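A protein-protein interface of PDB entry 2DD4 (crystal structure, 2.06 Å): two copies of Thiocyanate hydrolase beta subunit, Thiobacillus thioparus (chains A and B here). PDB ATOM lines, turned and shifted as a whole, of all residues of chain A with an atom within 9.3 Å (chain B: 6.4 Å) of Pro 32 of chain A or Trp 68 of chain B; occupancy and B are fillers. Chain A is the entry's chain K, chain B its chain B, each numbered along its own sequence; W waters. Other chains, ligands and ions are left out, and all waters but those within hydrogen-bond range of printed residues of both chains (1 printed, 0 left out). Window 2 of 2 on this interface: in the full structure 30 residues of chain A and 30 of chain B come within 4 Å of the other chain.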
ATOM      1  N   ALA A  29     -10.077   1.221 -18.650  1.00  0.00           N
ATOM      2  CA  ALA A  29      -9.913   2.417 -19.471  1.00  0.00           C
ATOM      3  C   ALA A  29     -10.121   2.122 -20.959  1.00  0.00           C
ATOM      4  O   ALA A  29      -9.218   2.322 -21.770  1.00  0.00           O
ATOM      5  CB  ALA A  29      -8.514   3.004 -19.244  1.00  0.00           C
ATOM      6  N   PRO A  30     -11.317   1.648 -21.337  1.00  0.00           N
ATOM      7  CA  PRO A  30     -11.595   1.341 -22.742  1.00  0.00           C
ATOM      8  C   PRO A  30     -11.570   2.579 -23.636  1.00  0.00           C
ATOM      9  O   PRO A  30     -11.771   3.703 -23.168  1.00  0.00           O
ATOM     10  CB  PRO A  30     -12.975   0.683 -22.684  1.00  0.00           C
ATOM     11  CG  PRO A  30     -13.611   1.345 -21.508  1.00  0.00           C
ATOM     12  CD  PRO A  30     -12.496   1.374 -20.494  1.00  0.00           C
ATOM     13  N   ALA A  31     -11.313   2.358 -24.921  1.00  0.00           N
ATOM     14  CA  ALA A  31     -11.255   3.436 -25.903  1.00  0.00           C
ATOM     15  C   ALA A  31     -12.628   4.077 -26.098  1.00  0.00           C
ATOM     16  O   ALA A  31     -13.658   3.441 -25.868  1.00  0.00           O
ATOM     17  CB  ALA A  31     -10.745   2.890 -27.234  1.00  0.00           C
ATOM     18  N   PRO A  32     -12.657   5.346 -26.535  1.00  0.00           N
ATOM     19  CA  PRO A  32     -13.904   6.078 -26.768  1.00  0.00           C
ATOM     20  C   PRO A  32     -14.879   5.293 -27.648  1.00  0.00           C
ATOM     21  O   PRO A  32     -16.093   5.391 -27.486  1.00  0.00           O
ATOM     22  CB  PRO A  32     -13.424   7.360 -27.441  1.00  0.00           C
ATOM     23  CG  PRO A  32     -12.103   7.595 -26.780  1.00  0.00           C
ATOM     24  CD  PRO A  32     -11.490   6.213 -26.791  1.00  0.00           C
ATOM     25  N   THR A  33     -14.336   4.512 -28.577  1.00  0.00           N
ATOM     26  CA  THR A  33     -15.151   3.713 -29.483  1.00  0.00           C
ATOM     27  C   THR A  33     -15.878   2.564 -28.784  1.00  0.00           C
ATOM     28  O   THR A  33     -16.736   1.915 -29.381  1.00  0.00           O
ATOM     29  CB  THR A  33     -14.293   3.140 -30.630  1.00  0.00           C
ATOM     30  OG1 THR A  33     -13.095   2.563 -30.094  1.00  0.00           O
ATOM     31  CG2 THR A  33     -13.922   4.235 -31.614  1.00  0.00           C
ATOM     32  N   GLU A  34     -15.538   2.313 -27.522  1.00  0.00           N
ATOM     33  CA  GLU A  34     -16.181   1.245 -26.758  1.00  0.00           C
ATOM     34  C   GLU A  34     -17.305   1.792 -25.888  1.00  0.00           C
ATOM     35  O   GLU A  34     -18.006   1.042 -25.211  1.00  0.00           O
ATOM     36  CB  GLU A  34     -15.159   0.533 -25.866  1.00  0.00           C
ATOM     37  CG  GLU A  34     -14.125  -0.254 -26.637  1.00  0.00           C
ATOM     38  CD  GLU A  34     -14.766  -1.259 -27.566  1.00  0.00           C
ATOM     39  OE1 GLU A  34     -15.454  -2.178 -27.066  1.00  0.00           O
ATOM     40  OE2 GLU A  34     -14.592  -1.127 -28.796  1.00  0.00           O
ATOM     41  N   ILE A  35     -17.476   3.106 -25.913  1.00  0.00           N
ATOM     42  CA  ILE A  35     -18.502   3.744 -25.109  1.00  0.00           C
ATOM     43  C   ILE A  35     -19.701   4.131 -25.965  1.00  0.00           C
ATOM     44  O   ILE A  35     -19.600   5.001 -26.825  1.00  0.00           O
ATOM     45  CB  ILE A  35     -17.943   5.015 -24.432  1.00  0.00           C
ATOM     46  CG1 ILE A  35     -16.694   4.662 -23.617  1.00  0.00           C
ATOM     47  CG2 ILE A  35     -19.011   5.652 -23.550  1.00  0.00           C
ATOM     48  CD1 ILE A  35     -16.940   3.646 -22.508  1.00  0.00           C
ATOM     49  N   THR A  36     -20.829   3.469 -25.737  1.00  0.00           N
ATOM     50  CA  THR A  36     -22.052   3.769 -26.469  1.00  0.00           C
ATOM     51  C   THR A  36     -22.727   4.911 -25.722  1.00  0.00           C
ATOM     52  O   THR A  36     -22.319   5.249 -24.609  1.00  0.00           O
ATOM     53  CB  THR A  36     -23.022   2.590 -26.454  1.00  0.00           C
ATOM     54  OG1 THR A  36     -23.265   2.206 -25.096  1.00  0.00           O
ATOM     55  CG2 THR A  36     -22.454   1.412 -27.226  1.00  0.00           C
ATOM     56  N   HIS A  37     -23.752   5.505 -26.324  1.00  0.00           N
ATOM     57  CA  HIS A  37     -24.459   6.580 -25.651  1.00  0.00           C
ATOM     58  C   HIS A  37     -25.058   6.051 -24.353  1.00  0.00           C
ATOM     59  O   HIS A  37     -25.057   6.741 -23.339  1.00  0.00           O
ATOM     60  CB  HIS A  37     -25.589   7.144 -26.513  1.00  0.00           C
ATOM     61  CG  HIS A  37     -26.500   8.058 -25.756  1.00  0.00           C
ATOM     62  ND1 HIS A  37     -26.067   9.243 -25.201  1.00  0.00           N
ATOM     63  CD2 HIS A  37     -27.794   7.917 -25.379  1.00  0.00           C
ATOM     64  CE1 HIS A  37     -27.052   9.792 -24.513  1.00  0.00           C
ATOM     65  NE2 HIS A  37     -28.110   9.006 -24.603  1.00  0.00           N
ATOM     66  N   LEU A  39     -23.955   3.689 -22.394  1.00  0.00           N
ATOM     67  CA  LEU A  39     -22.920   3.565 -21.376  1.00  0.00           C
ATOM     68  C   LEU A  39     -22.480   4.943 -20.901  1.00  0.00           C
ATOM     69  O   LEU A  39     -22.193   5.137 -19.720  1.00  0.00           O
ATOM     70  CB  LEU A  39     -21.716   2.792 -21.920  1.00  0.00           C
ATOM     71  CG  LEU A  39     -21.855   1.265 -21.965  1.00  0.00           C
ATOM     72  CD1 LEU A  39     -20.615   0.652 -22.619  1.00  0.00           C
ATOM     73  CD2 LEU A  39     -22.030   0.724 -20.554  1.00  0.00           C
ATOM     74  N   PHE A  40     -22.433   5.901 -21.821  1.00  0.00           N
ATOM     75  CA  PHE A  40     -22.032   7.255 -21.473  1.00  0.00           C
ATOM     76  C   PHE A  40     -22.999   7.804 -20.427  1.00  0.00           C
ATOM     77  O   PHE A  40     -22.578   8.388 -19.427  1.00  0.00           O
ATOM     78  CB  PHE A  40     -22.048   8.167 -22.706  1.00  0.00           C
ATOM     79  CG  PHE A  40     -21.536   9.558 -22.433  1.00  0.00           C
ATOM     80  CD1 PHE A  40     -20.187   9.863 -22.593  1.00  0.00           C
ATOM     81  CD2 PHE A  40     -22.398  10.555 -21.971  1.00  0.00           C
ATOM     82  CE1 PHE A  40     -19.699  11.138 -22.297  1.00  0.00           C
ATOM     83  CE2 PHE A  40     -21.924  11.833 -21.670  1.00  0.00           C
ATOM     84  CZ  PHE A  40     -20.568  12.126 -21.834  1.00  0.00           C
ATOM     85  N   LYS B  63      -3.161   3.802 -30.726  1.00  0.00           N
ATOM     86  CA  LYS B  63      -4.521   4.231 -31.046  1.00  0.00           C
ATOM     87  C   LYS B  63      -4.478   5.590 -31.725  1.00  0.00           C
ATOM     88  O   LYS B  63      -3.783   6.493 -31.266  1.00  0.00           O
ATOM     89  CB  LYS B  63      -5.401   4.324 -29.791  1.00  0.00           C
ATOM     90  CG  LYS B  63      -6.869   4.638 -30.117  1.00  0.00           C
ATOM     91  CD  LYS B  63      -7.740   4.882 -28.874  1.00  0.00           C
ATOM     92  CE  LYS B  63      -7.633   6.320 -28.372  1.00  0.00           C
ATOM     93  NZ  LYS B  63      -8.157   7.310 -29.369  1.00  0.00           N
ATOM     94  N   GLU B  65      -5.442   9.283 -32.726  1.00  0.00           N
ATOM     95  CA  GLU B  65      -6.013  10.357 -31.927  1.00  0.00           C
ATOM     96  C   GLU B  65      -7.338  10.792 -32.531  1.00  0.00           C
ATOM     97  O   GLU B  65      -7.443  10.965 -33.745  1.00  0.00           O
ATOM     98  CB  GLU B  65      -5.098  11.579 -31.903  1.00  0.00           C
ATOM     99  CG  GLU B  65      -3.745  11.371 -31.290  1.00  0.00           C
ATOM    100  CD  GLU B  65      -3.037  12.689 -31.024  1.00  0.00           C
ATOM    101  OE1 GLU B  65      -1.864  12.648 -30.595  1.00  0.00           O
ATOM    102  OE2 GLU B  65      -3.658  13.763 -31.238  1.00  0.00           O
ATOM    103  N   GLU B  66      -8.344  10.969 -31.683  1.00  0.00           N
ATOM    104  CA  GLU B  66      -9.647  11.435 -32.137  1.00  0.00           C
ATOM    105  C   GLU B  66      -9.507  12.945 -32.240  1.00  0.00           C
ATOM    106  O   GLU B  66      -8.725  13.552 -31.503  1.00  0.00           O
ATOM    107  CB  GLU B  66     -10.730  11.111 -31.105  1.00  0.00           C
ATOM    108  CG  GLU B  66     -11.065   9.635 -30.955  1.00  0.00           C
ATOM    109  CD  GLU B  66     -12.068   9.151 -31.984  1.00  0.00           C
ATOM    110  OE1 GLU B  66     -12.495   9.959 -32.839  1.00  0.00           O
ATOM    111  OE2 GLU B  66     -12.432   7.958 -31.933  1.00  0.00           O
ATOM    112  N   ILE B  67     -10.250  13.557 -33.152  1.00  0.00           N
ATOM    113  CA  ILE B  67     -10.199  15.006 -33.290  1.00  0.00           C
ATOM    114  C   ILE B  67     -10.558  15.639 -31.945  1.00  0.00           C
ATOM    115  O   ILE B  67      -9.910  16.588 -31.504  1.00  0.00           O
ATOM    116  CB  ILE B  67     -11.218  15.512 -34.332  1.00  0.00           C
ATOM    117  CG1 ILE B  67     -10.862  14.985 -35.725  1.00  0.00           C
ATOM    118  CG2 ILE B  67     -11.262  17.033 -34.310  1.00  0.00           C
ATOM    119  CD1 ILE B  67      -9.591  15.557 -36.281  1.00  0.00           C
ATOM    120  N   TRP B  68     -11.591  15.110 -31.291  1.00  0.00           N
ATOM    121  CA  TRP B  68     -12.012  15.672 -30.012  1.00  0.00           C
ATOM    122  C   TRP B  68     -10.981  15.494 -28.900  1.00  0.00           C
ATOM    123  O   TRP B  68     -10.921  16.299 -27.966  1.00  0.00           O
ATOM    124  CB  TRP B  68     -13.379  15.109 -29.580  1.00  0.00           C
ATOM    125  CG  TRP B  68     -13.396  13.679 -29.108  1.00  0.00           C
ATOM    126  CD1 TRP B  68     -13.690  12.569 -29.852  1.00  0.00           C
ATOM    127  CD2 TRP B  68     -13.152  13.214 -27.772  1.00  0.00           C
ATOM    128  NE1 TRP B  68     -13.649  11.445 -29.060  1.00  0.00           N
ATOM    129  CE2 TRP B  68     -13.323  11.812 -27.780  1.00  0.00           C
ATOM    130  CE3 TRP B  68     -12.811  13.848 -26.570  1.00  0.00           C
ATOM    131  CZ2 TRP B  68     -13.162  11.028 -26.628  1.00  0.00           C
ATOM    132  CZ3 TRP B  68     -12.649  13.067 -25.422  1.00  0.00           C
ATOM    133  CH2 TRP B  68     -12.827  11.671 -25.464  1.00  0.00           C
ATOM    134  N   GLU B  69     -10.159  14.451 -28.998  1.00  0.00           N
ATOM    135  CA  GLU B  69      -9.128  14.215 -27.994  1.00  0.00           C
ATOM    136  C   GLU B  69      -8.057  15.302 -28.109  1.00  0.00           C
ATOM    137  O   GLU B  69      -7.586  15.840 -27.101  1.00  0.00           O
ATOM    138  CB  GLU B  69      -8.499  12.827 -28.179  1.00  0.00           C
ATOM    139  CG  GLU B  69      -9.458  11.661 -27.907  1.00  0.00           C
ATOM    140  CD  GLU B  69      -8.789  10.299 -28.033  1.00  0.00           C
ATOM    141  OE1 GLU B  69      -8.026  10.105 -29.001  1.00  0.00           O
ATOM    142  OE2 GLU B  69      -9.034   9.420 -27.175  1.00  0.00           O
ATOM    143  N   LEU B  70      -7.674  15.630 -29.342  1.00  0.00           N
ATOM    144  CA  LEU B  70      -6.675  16.667 -29.552  1.00  0.00           C
ATOM    145  C   LEU B  70      -7.227  18.004 -29.059  1.00  0.00           C
ATOM    146  O   LEU B  70      -6.517  18.778 -28.424  1.00  0.00           O
ATOM    147  CB  LEU B  70      -6.307  16.771 -31.035  1.00  0.00           C
ATOM    148  CG  LEU B  70      -5.475  18.008 -31.397  1.00  0.00           C
ATOM    149  CD1 LEU B  70      -4.198  18.039 -30.563  1.00  0.00           C
ATOM    150  CD2 LEU B  70      -5.147  17.985 -32.887  1.00  0.00           C
ATOM    151  N   ASN B  71      -8.497  18.271 -29.353  1.00  0.00           N
ATOM    152  CA  ASN B  71      -9.135  19.516 -28.927  1.00  0.00           C
ATOM    153  C   ASN B  71      -9.261  19.577 -27.408  1.00  0.00           C
ATOM    154  O   ASN B  71      -9.167  20.647 -26.811  1.00  0.00           O
ATOM    155  CB  ASN B  71     -10.518  19.640 -29.566  1.00  0.00           C
ATOM    156  CG  ASN B  71     -10.454  20.120 -31.007  1.00  0.00           C
ATOM    157  OD1 ASN B  71     -11.358  19.857 -31.798  1.00  0.00           O
ATOM    158  ND2 ASN B  71      -9.392  20.842 -31.349  1.00  0.00           N
ATOM    159  N   THR B  72      -9.470  18.420 -26.787  1.00  0.00           N
ATOM    160  CA  THR B  72      -9.600  18.349 -25.336  1.00  0.00           C
ATOM    161  C   THR B  72      -8.253  18.642 -24.692  1.00  0.00           C
ATOM    162  O   THR B  72      -8.168  19.394 -23.720  1.00  0.00           O
ATOM    163  CB  THR B  72     -10.093  16.955 -24.887  1.00  0.00           C
ATOM    164  OG1 THR B  72     -11.418  16.738 -25.387  1.00  0.00           O
ATOM    165  CG2 THR B  72     -10.107  16.850 -23.359  1.00  0.00           C
ATOM    166  N   PHE B  73      -7.199  18.046 -25.240  1.00  0.00           N
ATOM    167  CA  PHE B  73      -5.854  18.255 -24.720  1.00  0.00           C
ATOM    168  C   PHE B  73      -5.507  19.745 -24.764  1.00  0.00           C
ATOM    169  O   PHE B  73      -5.067  20.319 -23.769  1.00  0.00           O
ATOM    170  CB  PHE B  73      -4.839  17.456 -25.548  1.00  0.00           C
ATOM    171  CG  PHE B  73      -3.416  17.640 -25.105  1.00  0.00           C
ATOM    172  CD1 PHE B  73      -3.006  17.227 -23.841  1.00  0.00           C
ATOM    173  CD2 PHE B  73      -2.483  18.236 -25.950  1.00  0.00           C
ATOM    174  CE1 PHE B  73      -1.692  17.403 -23.422  1.00  0.00           C
ATOM    175  CE2 PHE B  73      -1.163  18.417 -25.539  1.00  0.00           C
ATOM    176  CZ  PHE B  73      -0.767  18.000 -24.272  1.00  0.00           C
ATOM    177  N   PRO B 107     -13.080   6.295 -20.882  1.00  0.00           N
ATOM    178  CA  PRO B 107     -11.804   6.460 -21.587  1.00  0.00           C
ATOM    179  C   PRO B 107     -10.909   7.552 -21.002  1.00  0.00           C
ATOM    180  O   PRO B 107     -11.382   8.515 -20.396  1.00  0.00           O
ATOM    181  CB  PRO B 107     -12.232   6.808 -23.019  1.00  0.00           C
ATOM    182  CG  PRO B 107     -13.662   6.320 -23.112  1.00  0.00           C
ATOM    183  CD  PRO B 107     -14.203   6.672 -21.756  1.00  0.00           C
ATOM    184  N   TYR B 108      -9.609   7.378 -21.207  1.00  0.00           N
ATOM    185  CA  TYR B 108      -8.571   8.313 -20.778  1.00  0.00           C
ATOM    186  C   TYR B 108      -8.987   9.769 -21.034  1.00  0.00           C
ATOM    187  O   TYR B 108      -9.164  10.545 -20.096  1.00  0.00           O
ATOM    188  CB  TYR B 108      -7.297   7.985 -21.560  1.00  0.00           C
ATOM    189  CG  TYR B 108      -6.123   8.931 -21.408  1.00  0.00           C
ATOM    190  CD1 TYR B 108      -5.284   8.864 -20.297  1.00  0.00           C
ATOM    191  CD2 TYR B 108      -5.789   9.820 -22.436  1.00  0.00           C
ATOM    192  CE1 TYR B 108      -4.133   9.648 -20.218  1.00  0.00           C
ATOM    193  CE2 TYR B 108      -4.641  10.609 -22.365  1.00  0.00           C
ATOM    194  CZ  TYR B 108      -3.818  10.513 -21.259  1.00  0.00           C
ATOM    195  OH  TYR B 108      -2.667  11.260 -21.209  1.00  0.00           O
ATOM    196  N   TYR B 109      -9.146  10.137 -22.306  1.00  0.00           N
ATOM    197  CA  TYR B 109      -9.526  11.506 -22.643  1.00  0.00           C
ATOM    198  C   TYR B 109     -10.957  11.867 -22.258  1.00  0.00           C
ATOM    199  O   TYR B 109     -11.311  13.046 -22.199  1.00  0.00           O
ATOM    200  CB  TYR B 109      -9.274  11.780 -24.131  1.00  0.00           C
ATOM    201  CG  TYR B 109      -7.889  12.346 -24.380  1.00  0.00           C
ATOM    202  CD1 TYR B 109      -6.999  11.723 -25.254  1.00  0.00           C
ATOM    203  CD2 TYR B 109      -7.465  13.504 -23.724  1.00  0.00           C
ATOM    204  CE1 TYR B 109      -5.717  12.241 -25.466  1.00  0.00           C
ATOM    205  CE2 TYR B 109      -6.189  14.028 -23.926  1.00  0.00           C
ATOM    206  CZ  TYR B 109      -5.322  13.391 -24.799  1.00  0.00           C
ATOM    207  OH  TYR B 109      -4.071  13.911 -25.004  1.00  0.00           O
ATOM    208  N   GLY B 110     -11.776  10.855 -21.995  1.00  0.00           N
ATOM    209  CA  GLY B 110     -13.138  11.121 -21.576  1.00  0.00           C
ATOM    210  C   GLY B 110     -13.061  11.780 -20.208  1.00  0.00           C
ATOM    211  O   GLY B 110     -13.819  12.699 -19.897  1.00  0.00           O
ATOM    212  N   ARG B 111     -12.125  11.308 -19.387  1.00  0.00           N
ATOM    213  CA  ARG B 111     -11.937  11.865 -18.053  1.00  0.00           C
ATOM    214  C   ARG B 111     -11.347  13.274 -18.144  1.00  0.00           C
ATOM    215  O   ARG B 111     -11.720  14.160 -17.373  1.00  0.00           O
ATOM    216  CB  ARG B 111     -11.039  10.942 -17.217  1.00  0.00           C
ATOM    217  CG  ARG B 111     -11.666   9.564 -16.982  1.00  0.00           C
ATOM    218  CD  ARG B 111     -10.855   8.671 -16.033  1.00  0.00           C
ATOM    219  NE  ARG B 111      -9.540   8.310 -16.555  1.00  0.00           N
ATOM    220  CZ  ARG B 111      -8.409   8.948 -16.265  1.00  0.00           C
ATOM    221  NH1 ARG B 111      -8.415   9.996 -15.451  1.00  0.00           N
ATOM    222  NH2 ARG B 111      -7.260   8.527 -16.781  1.00  0.00           N
ATOM    223  N   LEU B 113     -11.806  15.465 -20.520  1.00  0.00           N
ATOM    224  CA  LEU B 113     -12.910  16.319 -20.951  1.00  0.00           C
ATOM    225  C   LEU B 113     -13.926  16.578 -19.849  1.00  0.00           C
ATOM    226  O   LEU B 113     -14.306  17.721 -19.609  1.00  0.00           O
ATOM    227  CB  LEU B 113     -13.609  15.704 -22.166  1.00  0.00           C
ATOM    228  CG  LEU B 113     -14.810  16.477 -22.726  1.00  0.00           C
ATOM    229  CD1 LEU B 113     -14.386  17.889 -23.096  1.00  0.00           C
ATOM    230  CD2 LEU B 113     -15.369  15.749 -23.940  1.00  0.00           C
ATOM    231  N   TYR B 151     -16.346  18.285 -36.640  1.00  0.00           N
ATOM    232  CA  TYR B 151     -16.846  16.939 -36.393  1.00  0.00           C
ATOM    233  C   TYR B 151     -17.937  16.546 -37.374  1.00  0.00           C
ATOM    234  O   TYR B 151     -18.017  15.392 -37.800  1.00  0.00           O
ATOM    235  CB  TYR B 151     -17.398  16.830 -34.970  1.00  0.00           C
ATOM    236  CG  TYR B 151     -16.403  17.193 -33.896  1.00  0.00           C
ATOM    237  CD1 TYR B 151     -16.633  18.271 -33.042  1.00  0.00           C
ATOM    238  CD2 TYR B 151     -15.229  16.456 -33.728  1.00  0.00           C
ATOM    239  CE1 TYR B 151     -15.721  18.608 -32.045  1.00  0.00           C
ATOM    240  CE2 TYR B 151     -14.310  16.784 -32.735  1.00  0.00           C
ATOM    241  CZ  TYR B 151     -14.560  17.859 -31.897  1.00  0.00           C
ATOM    242  OH  TYR B 151     -13.653  18.189 -30.914  1.00  0.00           O
HETATM  243  O   HOH W   1      -8.589   5.036 -22.393  1.00  0.00           O
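The side-chain amino group of Lys 63 of chain B lies within salt-bridge range of the side-chain carboxylate of Glu 69 of chain B (2.8 Å). The backbone NH (N) of Glu 66 of chain B sits at hydrogen-bond distance from the side-chain carboxylate (OE1) of Glu 69 of chain B. O of Trp 68 of chain B lies within hydrogen-bond range of OG1 of Thr 72 of chain B (2.7 Å).
Among the printed residues, merely in contact across the chains: Pro 30 of chain A with Pro 107 of chain B (3.1 Å), Ile 35 of chain A with Pro 107 of chain B (3.5 Å), Pro 32 of chain A with Glu 69 of chain B (3.6 Å), Pro 32 of chain A with Trp 68 of chain B (3.6 Å), Pro 32 of chain A with Pro 107 of chain B (3.7 Å), Ala 31 of chain A with Pro 107 of chain B (3.9 Å) and Ala 31 of chain A with Lys 63 of chain B (3.96 Å).
Printed residues of chain B within 4 Å of Pro 30 of chain A: Pro 107 (3.1 Å). Printed residues of chain B within 4 Å of Ile 35 of chain A: Pro 107 (3.5 Å). Of chain A, only Pro 32 comes within 4 Å of Trp 68 of chain B. Phe 73 of chain B touches none of the printed residues of chain A. Printed residues of chain A within 4 Å of Pro 107 of chain B: Pro 30 (3.1 Å), Ala 31 (3.9 Å), Pro 32 (3.7 Å) and Ile 35 (3.5 Å). Tyr 108 of chain B touches none of the printed residues of chain A. The nearest printed residue of chain B that does not touch Ala 31 of chain A is Tyr 108 of chain B (6.3 Å).
Of the 11 printed residues of chain A, 4 touch a printed residue of chain B. Printed residues of chain A that touch a printed residue of chain B: Pro 30, Ala 31, Pro 32 and Ile 35. Hydrophobic or aromatic side chains of chain A within 4 Å of the printed part of chain B: Ala 31, Pro 32 and Ile 35. Of the 17 printed residues of chain B, 4 touch a printed residue of chain A. Hydrophobic or aromatic side chains of chain B within 4 Å of the printed part of chain A: Trp 68 and Pro 107. Among the printed residues, 7 pairs touch across the chains. Among the printed residues, no Asp or Glu carboxylate lies within 4 Å of a Lys or Arg side-chain nitrogen of the other chain.
No position is printed for both chains. Of the 7 pairs that touch across the chains among the printed residues, none has its exchanged pair printed and touching as well.
Water W1 bridges N of Tyr 108 of chain B and O of Ala 29 of chain A.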
